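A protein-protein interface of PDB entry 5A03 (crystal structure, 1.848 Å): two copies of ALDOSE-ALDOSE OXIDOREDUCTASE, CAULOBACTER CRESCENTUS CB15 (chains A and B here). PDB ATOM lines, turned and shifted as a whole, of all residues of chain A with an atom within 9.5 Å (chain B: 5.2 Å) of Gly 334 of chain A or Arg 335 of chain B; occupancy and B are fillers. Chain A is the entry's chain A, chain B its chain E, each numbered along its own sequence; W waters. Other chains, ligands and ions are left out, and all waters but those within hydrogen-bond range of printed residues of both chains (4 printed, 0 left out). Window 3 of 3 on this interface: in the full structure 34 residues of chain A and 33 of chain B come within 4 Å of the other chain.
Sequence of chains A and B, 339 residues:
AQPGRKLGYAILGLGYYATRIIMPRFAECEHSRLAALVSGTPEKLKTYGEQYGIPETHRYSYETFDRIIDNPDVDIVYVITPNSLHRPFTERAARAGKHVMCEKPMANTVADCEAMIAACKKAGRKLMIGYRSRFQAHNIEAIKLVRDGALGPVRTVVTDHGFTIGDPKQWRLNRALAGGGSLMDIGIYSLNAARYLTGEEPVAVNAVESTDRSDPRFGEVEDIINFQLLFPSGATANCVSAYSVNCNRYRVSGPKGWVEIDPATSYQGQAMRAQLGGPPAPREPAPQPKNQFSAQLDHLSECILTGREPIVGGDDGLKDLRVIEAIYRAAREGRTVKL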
ATOM      1  N   VAL A 205      -0.358  11.671 -10.295  1.00  0.00           N
ATOM      2  CA  VAL A 205      -0.845  11.095  -9.049  1.00  0.00           C
ATOM      3  C   VAL A 205      -2.358  11.268  -8.891  1.00  0.00           C
ATOM      4  O   VAL A 205      -2.875  12.385  -9.062  1.00  0.00           O
ATOM      5  CB  VAL A 205      -0.144  11.754  -7.841  1.00  0.00           C
ATOM      6  CG1 VAL A 205      -0.630  11.158  -6.535  1.00  0.00           C
ATOM      7  CG2 VAL A 205       1.376  11.606  -7.962  1.00  0.00           C
ATOM      8  N   ASN A 206      -3.056  10.172  -8.585  1.00  0.00           N
ATOM      9  CA  ASN A 206      -4.445  10.189  -8.102  1.00  0.00           C
ATOM     10  C   ASN A 206      -4.477   9.733  -6.652  1.00  0.00           C
ATOM     11  O   ASN A 206      -3.607   8.984  -6.222  1.00  0.00           O
ATOM     12  CB  ASN A 206      -5.361   9.241  -8.896  1.00  0.00           C
ATOM     13  CG  ASN A 206      -5.825   9.812 -10.221  1.00  0.00           C
ATOM     14  OD1 ASN A 206      -5.915  11.027 -10.407  1.00  0.00           O
ATOM     15  ND2 ASN A 206      -6.146   8.916 -11.155  1.00  0.00           N
ATOM     16  N   ALA A 207      -5.505  10.113  -5.913  1.00  0.00           N
ATOM     17  CA  ALA A 207      -5.636   9.616  -4.550  1.00  0.00           C
ATOM     18  C   ALA A 207      -7.072   9.711  -4.073  1.00  0.00           C
ATOM     19  O   ALA A 207      -7.835  10.583  -4.515  1.00  0.00           O
ATOM     20  CB  ALA A 207      -4.706  10.383  -3.610  1.00  0.00           C
ATOM     21  N   VAL A 208      -7.442   8.789  -3.190  1.00  0.00           N
ATOM     22  CA  VAL A 208      -8.725   8.845  -2.500  1.00  0.00           C
ATOM     23  C   VAL A 208      -8.473   8.648  -1.013  1.00  0.00           C
ATOM     24  O   VAL A 208      -7.746   7.731  -0.613  1.00  0.00           O
ATOM     25  CB  VAL A 208      -9.742   7.773  -3.014  1.00  0.00           C
ATOM     26  CG1 VAL A 208     -10.077   7.995  -4.480  1.00  0.00           C
ATOM     27  CG2 VAL A 208      -9.205   6.391  -2.850  1.00  0.00           C
ATOM     28  N   GLU A 209      -9.059   9.510  -0.192  1.00  0.00           N
ATOM     29  CA  GLU A 209      -8.932   9.374   1.256  1.00  0.00           C
ATOM     30  C   GLU A 209     -10.228   8.847   1.848  1.00  0.00           C
ATOM     31  O   GLU A 209     -11.313   9.127   1.339  1.00  0.00           O
ATOM     32  CB  GLU A 209      -8.557  10.712   1.904  1.00  0.00           C
ATOM     33  CG  GLU A 209      -8.244  10.572   3.376  1.00  0.00           C
ATOM     34  CD  GLU A 209      -8.669  11.775   4.183  1.00  0.00           C
ATOM     35  OE1 GLU A 209      -8.478  12.915   3.700  1.00  0.00           O
ATOM     36  OE2 GLU A 209      -9.185  11.576   5.306  1.00  0.00           O
ATOM     37  N   GLN A 228      -2.676   6.319  -6.822  1.00  0.00           N
ATOM     38  CA  GLN A 228      -2.186   5.791  -8.092  1.00  0.00           C
ATOM     39  C   GLN A 228      -1.033   6.640  -8.572  1.00  0.00           C
ATOM     40  O   GLN A 228      -1.078   7.872  -8.451  1.00  0.00           O
ATOM     41  CB  GLN A 228      -3.283   5.807  -9.146  1.00  0.00           C
ATOM     42  CG  GLN A 228      -4.538   5.074  -8.724  1.00  0.00           C
ATOM     43  CD  GLN A 228      -5.554   5.029  -9.845  1.00  0.00           C
ATOM     44  OE1 GLN A 228      -6.108   6.061 -10.242  1.00  0.00           O
ATOM     45  NE2 GLN A 228      -5.788   3.835 -10.385  1.00  0.00           N
ATOM     46  N   ALA A 326       1.825  15.756  -3.231  1.00  0.00           N
ATOM     47  CA  ALA A 326       0.943  15.606  -4.389  1.00  0.00           C
ATOM     48  C   ALA A 326      -0.208  14.634  -4.116  1.00  0.00           C
ATOM     49  O   ALA A 326      -1.334  14.841  -4.571  1.00  0.00           O
ATOM     50  CB  ALA A 326       1.747  15.151  -5.623  1.00  0.00           C
ATOM     51  N   ILE A 327       0.081  13.551  -3.402  1.00  0.00           N
ATOM     52  CA  ILE A 327      -0.955  12.605  -2.994  1.00  0.00           C
ATOM     53  C   ILE A 327      -2.023  13.292  -2.131  1.00  0.00           C
ATOM     54  O   ILE A 327      -3.227  13.186  -2.414  1.00  0.00           O
ATOM     55  CB  ILE A 327      -0.323  11.393  -2.244  1.00  0.00           C
ATOM     56  CG1 ILE A 327       0.491  10.559  -3.238  1.00  0.00           C
ATOM     57  CG2 ILE A 327      -1.396  10.522  -1.579  1.00  0.00           C
ATOM     58  CD1 ILE A 327       1.505   9.586  -2.539  1.00  0.00           C
ATOM     59  N   TYR A 328      -1.595  14.008  -1.093  1.00  0.00           N
ATOM     60  CA  TYR A 328      -2.550  14.736  -0.257  1.00  0.00           C
ATOM     61  C   TYR A 328      -3.353  15.735  -1.095  1.00  0.00           C
ATOM     62  O   TYR A 328      -4.555  15.885  -0.900  1.00  0.00           O
ATOM     63  CB  TYR A 328      -1.835  15.469   0.880  1.00  0.00           C
ATOM     64  CG  TYR A 328      -1.404  14.576   2.031  1.00  0.00           C
ATOM     65  CD1 TYR A 328      -2.283  13.647   2.595  1.00  0.00           C
ATOM     66  CD2 TYR A 328      -0.128  14.677   2.566  1.00  0.00           C
ATOM     67  CE1 TYR A 328      -1.890  12.824   3.660  1.00  0.00           C
ATOM     68  CE2 TYR A 328       0.273  13.866   3.626  1.00  0.00           C
ATOM     69  CZ  TYR A 328      -0.610  12.946   4.173  1.00  0.00           C
ATOM     70  OH  TYR A 328      -0.195  12.153   5.238  1.00  0.00           O
ATOM     71  N   ARG A 329      -2.687  16.388  -2.040  1.00  0.00           N
ATOM     72  CA  ARG A 329      -3.371  17.376  -2.888  1.00  0.00           C
ATOM     73  C   ARG A 329      -4.391  16.712  -3.811  1.00  0.00           C
ATOM     74  O   ARG A 329      -5.509  17.195  -3.982  1.00  0.00           O
ATOM     75  CB  ARG A 329      -2.359  18.168  -3.709  1.00  0.00           C
ATOM     76  CG  ARG A 329      -2.975  19.258  -4.581  1.00  0.00           C
ATOM     77  CD  ARG A 329      -1.885  20.144  -5.177  1.00  0.00           C
ATOM     78  NE  ARG A 329      -2.454  21.131  -6.088  1.00  0.00           N
ATOM     79  CZ  ARG A 329      -1.778  22.156  -6.606  1.00  0.00           C
ATOM     80  NH1 ARG A 329      -0.497  22.329  -6.305  1.00  0.00           N
ATOM     81  NH2 ARG A 329      -2.386  23.010  -7.425  1.00  0.00           N
ATOM     82  N   ALA A 330      -3.992  15.601  -4.409  1.00  0.00           N
ATOM     83  CA  ALA A 330      -4.860  14.878  -5.325  1.00  0.00           C
ATOM     84  C   ALA A 330      -6.143  14.440  -4.627  1.00  0.00           C
ATOM     85  O   ALA A 330      -7.223  14.510  -5.207  1.00  0.00           O
ATOM     86  CB  ALA A 330      -4.121  13.673  -5.906  1.00  0.00           C
ATOM     87  N   ALA A 331      -6.019  13.999  -3.377  1.00  0.00           N
ATOM     88  CA  ALA A 331      -7.188  13.576  -2.597  1.00  0.00           C
ATOM     89  C   ALA A 331      -8.052  14.773  -2.207  1.00  0.00           C
ATOM     90  O   ALA A 331      -9.281  14.730  -2.287  1.00  0.00           O
ATOM     91  CB  ALA A 331      -6.749  12.811  -1.355  1.00  0.00           C
ATOM     92  N   ARG A 332      -7.396  15.852  -1.808  1.00  0.00           N
ATOM     93  CA  ARG A 332      -8.094  17.075  -1.414  1.00  0.00           C
ATOM     94  C   ARG A 332      -8.854  17.692  -2.589  1.00  0.00           C
ATOM     95  O   ARG A 332     -10.022  18.092  -2.460  1.00  0.00           O
ATOM     96  CB  ARG A 332      -7.076  18.077  -0.832  1.00  0.00           C
ATOM     97  CG  ARG A 332      -7.647  19.393  -0.352  1.00  0.00           C
ATOM     98  CD  ARG A 332      -6.603  20.179   0.478  1.00  0.00           C
ATOM     99  NE  ARG A 332      -5.357  20.445  -0.248  1.00  0.00           N
ATOM    100  CZ  ARG A 332      -4.159  19.960   0.091  1.00  0.00           C
ATOM    101  NH1 ARG A 332      -4.028  19.179   1.158  1.00  0.00           N
ATOM    102  NH2 ARG A 332      -3.078  20.262  -0.632  1.00  0.00           N
ATOM    103  N   GLU A 333      -8.194  17.765  -3.739  1.00  0.00           N
ATOM    104  CA  GLU A 333      -8.781  18.431  -4.909  1.00  0.00           C
ATOM    105  C   GLU A 333      -9.573  17.512  -5.837  1.00  0.00           C
ATOM    106  O   GLU A 333     -10.256  17.989  -6.747  1.00  0.00           O
ATOM    107  CB  GLU A 333      -7.680  19.128  -5.700  1.00  0.00           C
ATOM    108  CG  GLU A 333      -7.005  20.210  -4.859  1.00  0.00           C
ATOM    109  CD  GLU A 333      -5.992  21.010  -5.625  1.00  0.00           C
ATOM    110  OE1 GLU A 333      -5.847  20.776  -6.839  1.00  0.00           O
ATOM    111  OE2 GLU A 333      -5.337  21.880  -5.006  1.00  0.00           O
ATOM    112  N   GLY A 334      -9.501  16.205  -5.598  1.00  0.00           N
ATOM    113  CA  GLY A 334     -10.203  15.244  -6.432  1.00  0.00           C
ATOM    114  C   GLY A 334      -9.826  15.367  -7.898  1.00  0.00           C
ATOM    115  O   GLY A 334     -10.687  15.390  -8.787  1.00  0.00           O
ATOM    116  N   ARG A 335      -8.531  15.473  -8.159  1.00  0.00           N
ATOM    117  CA  ARG A 335      -8.049  15.546  -9.530  1.00  0.00           C
ATOM    118  C   ARG A 335      -6.666  14.929  -9.631  1.00  0.00           C
ATOM    119  O   ARG A 335      -5.980  14.753  -8.621  1.00  0.00           O
ATOM    120  CB  ARG A 335      -8.019  16.991 -10.026  1.00  0.00           C
ATOM    121  CG  ARG A 335      -6.886  17.780  -9.452  1.00  0.00           C
ATOM    122  CD  ARG A 335      -6.791  19.208 -10.013  1.00  0.00           C
ATOM    123  NE  ARG A 335      -5.776  19.951  -9.259  1.00  0.00           N
ATOM    124  CZ  ARG A 335      -4.474  19.967  -9.546  1.00  0.00           C
ATOM    125  NH1 ARG A 335      -4.004  19.307 -10.603  1.00  0.00           N
ATOM    126  NH2 ARG A 335      -3.638  20.663  -8.782  1.00  0.00           N
ATOM    127  N   THR A 336      -6.249  14.609 -10.850  1.00  0.00           N
ATOM    128  CA  THR A 336      -4.921  14.066 -11.064  1.00  0.00           C
ATOM    129  C   THR A 336      -3.895  15.188 -10.901  1.00  0.00           C
ATOM    130  O   THR A 336      -4.008  16.240 -11.535  1.00  0.00           O
ATOM    131  CB  THR A 336      -4.776  13.428 -12.460  1.00  0.00           C
ATOM    132  OG1 THR A 336      -5.778  12.422 -12.637  1.00  0.00           O
ATOM    133  CG2 THR A 336      -3.418  12.778 -12.591  1.00  0.00           C
ATOM    134  N   VAL A 337      -2.899  14.974 -10.051  1.00  0.00           N
ATOM    135  CA  VAL A 337      -1.859  15.972  -9.869  1.00  0.00           C
ATOM    136  C   VAL A 337      -0.639  15.599 -10.695  1.00  0.00           C
ATOM    137  O   VAL A 337      -0.143  14.463 -10.649  1.00  0.00           O
ATOM    138  CB  VAL A 337      -1.456  16.137  -8.384  1.00  0.00           C
ATOM    139  CG1 VAL A 337      -0.220  17.039  -8.263  1.00  0.00           C
ATOM    140  CG2 VAL A 337      -2.614  16.718  -7.582  1.00  0.00           C
ATOM    141  N   VAL B 205     -14.815   7.805  -8.350  1.00  0.00           N
ATOM    142  CA  VAL B 205     -13.957   7.004  -9.219  1.00  0.00           C
ATOM    143  C   VAL B 205     -12.739   7.809  -9.650  1.00  0.00           C
ATOM    144  O   VAL B 205     -12.896   8.933 -10.145  1.00  0.00           O
ATOM    145  CB  VAL B 205     -14.711   6.546 -10.495  1.00  0.00           C
ATOM    146  CG1 VAL B 205     -13.793   5.746 -11.419  1.00  0.00           C
ATOM    147  CG2 VAL B 205     -15.966   5.766 -10.141  1.00  0.00           C
ATOM    148  N   ASN B 206     -11.543   7.244  -9.440  1.00  0.00           N
ATOM    149  CA  ASN B 206     -10.300   7.718 -10.055  1.00  0.00           C
ATOM    150  C   ASN B 206      -9.805   6.706 -11.064  1.00  0.00           C
ATOM    151  O   ASN B 206     -10.022   5.512 -10.888  1.00  0.00           O
ATOM    152  CB  ASN B 206      -9.182   7.931  -9.028  1.00  0.00           C
ATOM    153  CG  ASN B 206      -9.245   9.286  -8.367  1.00  0.00           C
ATOM    154  OD1 ASN B 206      -9.818  10.233  -8.909  1.00  0.00           O
ATOM    155  ND2 ASN B 206      -8.647   9.390  -7.189  1.00  0.00           N
ATOM    156  N   ARG B 329     -14.036   7.966 -18.123  1.00  0.00           N
ATOM    157  CA  ARG B 329     -14.112   9.432 -18.062  1.00  0.00           C
ATOM    158  C   ARG B 329     -13.070   9.999 -17.100  1.00  0.00           C
ATOM    159  O   ARG B 329     -12.484  11.036 -17.365  1.00  0.00           O
ATOM    160  CB  ARG B 329     -15.510   9.897 -17.648  1.00  0.00           C
ATOM    161  CG  ARG B 329     -15.618  11.426 -17.403  1.00  0.00           C
ATOM    162  CD  ARG B 329     -17.076  11.900 -17.363  1.00  0.00           C
ATOM    163  NE  ARG B 329     -17.808  11.385 -18.519  1.00  0.00           N
ATOM    164  CZ  ARG B 329     -18.090  12.096 -19.609  1.00  0.00           C
ATOM    165  NH1 ARG B 329     -17.721  13.375 -19.685  1.00  0.00           N
ATOM    166  NH2 ARG B 329     -18.750  11.535 -20.622  1.00  0.00           N
ATOM    167  N   ALA B 330     -12.863   9.321 -15.972  1.00  0.00           N
ATOM    168  CA  ALA B 330     -11.889   9.779 -14.979  1.00  0.00           C
ATOM    169  C   ALA B 330     -10.475   9.740 -15.542  1.00  0.00           C
ATOM    170  O   ALA B 330      -9.654  10.609 -15.249  1.00  0.00           O
ATOM    171  CB  ALA B 330     -11.992   8.917 -13.694  1.00  0.00           C
ATOM    172  N   GLU B 333     -10.306  12.637 -18.237  1.00  0.00           N
ATOM    173  CA  GLU B 333     -10.365  13.991 -17.696  1.00  0.00           C
ATOM    174  C   GLU B 333      -9.379  14.257 -16.561  1.00  0.00           C
ATOM    175  O   GLU B 333      -9.172  15.407 -16.173  1.00  0.00           O
ATOM    176  CB  GLU B 333     -11.787  14.287 -17.230  1.00  0.00           C
ATOM    177  CG  GLU B 333     -12.751  14.326 -18.417  1.00  0.00           C
ATOM    178  CD  GLU B 333     -14.162  14.683 -18.044  1.00  0.00           C
ATOM    179  OE1 GLU B 333     -14.403  15.047 -16.878  1.00  0.00           O
ATOM    180  OE2 GLU B 333     -15.040  14.596 -18.935  1.00  0.00           O
ATOM    181  N   GLY B 334      -8.780  13.196 -16.032  1.00  0.00           N
ATOM    182  CA  GLY B 334      -7.840  13.329 -14.932  1.00  0.00           C
ATOM    183  C   GLY B 334      -8.475  13.972 -13.717  1.00  0.00           C
ATOM    184  O   GLY B 334      -7.925  14.892 -13.122  1.00  0.00           O
ATOM    185  N   ARG B 335      -9.662  13.507 -13.359  1.00  0.00           N
ATOM    186  CA  ARG B 335     -10.329  14.023 -12.176  1.00  0.00           C
ATOM    187  C   ARG B 335     -11.154  12.922 -11.556  1.00  0.00           C
ATOM    188  O   ARG B 335     -11.444  11.917 -12.207  1.00  0.00           O
ATOM    189  CB  ARG B 335     -11.223  15.219 -12.516  1.00  0.00           C
ATOM    190  CG  ARG B 335     -12.400  14.831 -13.374  1.00  0.00           C
ATOM    191  CD  ARG B 335     -13.315  16.011 -13.693  1.00  0.00           C
ATOM    192  NE  ARG B 335     -14.447  15.570 -14.507  1.00  0.00           N
ATOM    193  CZ  ARG B 335     -15.604  15.118 -14.021  1.00  0.00           C
ATOM    194  NH1 ARG B 335     -15.808  15.054 -12.703  1.00  0.00           N
ATOM    195  NH2 ARG B 335     -16.565  14.732 -14.860  1.00  0.00           N
ATOM    196  N   THR B 336     -11.531  13.116 -10.298  1.00  0.00           N
ATOM    197  CA  THR B 336     -12.393  12.183  -9.607  1.00  0.00           C
ATOM    198  C   THR B 336     -13.815  12.340 -10.135  1.00  0.00           C
ATOM    199  O   THR B 336     -14.386  13.421 -10.069  1.00  0.00           O
ATOM    200  CB  THR B 336     -12.366  12.420  -8.080  1.00  0.00           C
ATOM    201  OG1 THR B 336     -11.008  12.359  -7.617  1.00  0.00           O
ATOM    202  CG2 THR B 336     -13.193  11.353  -7.356  1.00  0.00           C
ATOM    203  N   VAL B 337     -14.380  11.265 -10.670  1.00  0.00           N
ATOM    204  CA  VAL B 337     -15.759  11.298 -11.153  1.00  0.00           C
ATOM    205  C   VAL B 337     -16.722  10.852 -10.054  1.00  0.00           C
ATOM    206  O   VAL B 337     -16.526   9.812  -9.422  1.00  0.00           O
ATOM    207  CB  VAL B 337     -15.946  10.404 -12.389  1.00  0.00           C
ATOM    208  CG1 VAL B 337     -17.444  10.289 -12.760  1.00  0.00           C
ATOM    209  CG2 VAL B 337     -15.132  10.944 -13.544  1.00  0.00           C
ATOM    210  N   LYS B 338     -17.754  11.645  -9.812  1.00  0.00           N
ATOM    211  CA  LYS B 338     -18.708  11.317  -8.759  1.00  0.00           C
ATOM    212  C   LYS B 338     -19.898  10.579  -9.352  1.00  0.00           C
ATOM    213  O   LYS B 338     -20.355  10.911 -10.448  1.00  0.00           O
ATOM    214  CB  LYS B 338     -19.184  12.577  -8.026  1.00  0.00           C
ATOM    215  CG  LYS B 338     -18.085  13.567  -7.681  1.00  0.00           C
ATOM    216  CD  LYS B 338     -16.972  12.928  -6.852  1.00  0.00           C
ATOM    217  CE  LYS B 338     -17.224  13.060  -5.358  1.00  0.00           C
ATOM    218  NZ  LYS B 338     -17.398  14.491  -4.972  1.00  0.00           N
HETATM  219  O   HOH W   1     -10.506  11.641  -4.873  1.00  0.00           O
HETATM  220  O   HOH W   2      -8.785  10.091 -12.427  1.00  0.00           O
HETATM  221  O   HOH W   3      -8.351  12.235 -10.116  1.00  0.00           O
HETATM  222  O   HOH W   4      -7.327  12.164  -7.046  1.00  0.00           O
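ND2 of Asn 206 of chain B lies within hydrogen-bond range of O of Ala 207 of chain A, at 3.0 Å.
N of Thr 336 of chain A sits at hydrogen-bond distance from O of Gly 334 of chain B.
The backbone NH (N) of Thr 336 of chain B lies within hydrogen-bond range of the backbone carbonyl oxygen (O) of Gly 334 of chain A, at 2.9 Å.
OD1 of Asn 206 of chain A lies within hydrogen-bond range of OG1 of Thr 336 of chain A (2.6 Å).
The side-chain carboxylate (OE1) of Glu 333 of chain B is in salt-bridge range of the guanidinium group (NE) of Arg 335 of chain B (2.4 Å).
O of Ala 330 of chain B sits at hydrogen-bond distance from N of Arg 335 of chain B (3.5 Å).
The backbone carbonyl oxygen (O) of Ala 330 of chain A sits at hydrogen-bond distance from the backbone NH (N) of Arg 335 of chain A (3.4 Å).
OE1 of Glu 333 of chain A lies within salt-bridge range of NE of Arg 335 of chain A, at 2.6 Å.
The side-chain amide oxygen (OD1) of Asn 206 of chain B is in hydrogen-bond range of the side-chain hydroxyl (OG1) of Thr 336 of chain B (2.8 Å).
Among the printed residues, pairs that only touch across the chains: Asn 206 of chain A with Asn 206 of chain B (3.7 Å), Val 208 of chain A with Asn 206 of chain B (3.4 Å), Gln 228 of chain A with Asn 206 of chain B (3.8 Å), Gly 334 of chain A with Arg 335 of chain B (3.7 Å), Arg 335 of chain A with Gly 334 of chain B (3.7 Å) and Arg 335 of chain A with Arg 335 of chain B (3.8 Å).
Of the printed residues of chain B, Asn 206 of chain A touches Asn 206.
Of the printed residues of chain B, Val 208 of chain A touches Asn 206.
Gly 334 of chain A touches two residues of chain B.
Of the printed residues of chain A, Asn 206 of chain B touches Asn 206 (3.7 Å), Ala 207 (3.0 Å), Val 208 (3.4 Å) and Gln 228 (3.8 Å).
No residue of chain A comes within 4 Å of Ala 330 of chain B.
No residue of chain A comes within 4 Å of Glu 333 of chain B.
Of chain A, only Gly 334 (3.7 Å) and Arg 335 (3.8 Å) come within 4 Å of Arg 335 of chain B.
Of the printed residues of chain A, Thr 336 of chain B touches Gly 334.
The nearest printed residue of chain B that does not touch Gly 334 of chain A is Gly 334 of chain B (5.2 Å).
The nearest residue of chain A that does not touch Arg 335 of chain B is Thr 336 of chain A (4.1 Å).
The nearest printed residue of chain A that does not touch Thr 336 of chain B is Arg 335 of chain A (4.02 Å).
Of the 10 printed residues of chain B, 4 touch a printed residue of chain A.
Of the 18 printed residues of chain A, 7 touch a printed residue of chain B.
Hydrophobic or aromatic side chains of chain A that line the printed part of chain B: Val 208.
Among the printed residues, 9 pairs touch across the chains.
Among the printed residues, no Asp or Glu carboxylate lies within 4 Å of a Lys or Arg side-chain nitrogen of the other chain.
Asn 206 of chain A touches its own counterpart, Asn 206 of chain B.
Gly 334 of chain A touches Arg 335 of chain B, and with the chains exchanged Arg 335 of chain A touches Gly 334 of chain B.
Gly 334 of chain A touches Thr 336 of chain B, and with the chains exchanged Thr 336 of chain A touches Gly 334 of chain B.
Arg 335 of chain A touches its own counterpart, Arg 335 of chain B.
9 positions are printed for both chains.
Of the 9 pairs that touch across the chains among the printed residues, 6 have their exchanged pair printed and touching as well.
Water W3 lies within hydrogen-bond range of the side-chain amide oxygen (OD1) of Asn 206 of chain A (2.7 Å), the side-chain amide oxygen (OD1) of Asn 206 of chain B (2.8 Å), the backbone NH (N) of Thr 336 of chain A (3.3 Å) and the backbone NH (N) of Thr 336 of chain B (3.3 Å).
Water W1 bridges the side-chain hydroxyl of Thr 336 of chain B (2.9 Å) and the backbone carbonyl oxygen of Ala 207 of chain A (2.9 Å).
Water W4 lies within hydrogen-bond range of the backbone NH of Ala 207 of chain A, the backbone carbonyl oxygen of Ala 330 of chain A, the side-chain amide nitrogen of Asn 206 of chain B and the backbone carbonyl oxygen of Arg 335 of chain A.
Water W2 lies within hydrogen-bond range of the backbone carbonyl oxygen (O) of Ala 330 of chain B, the side-chain amide nitrogen (ND2) of Asn 206 of chain A and the backbone carbonyl oxygen (O) of Arg 335 of chain B.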
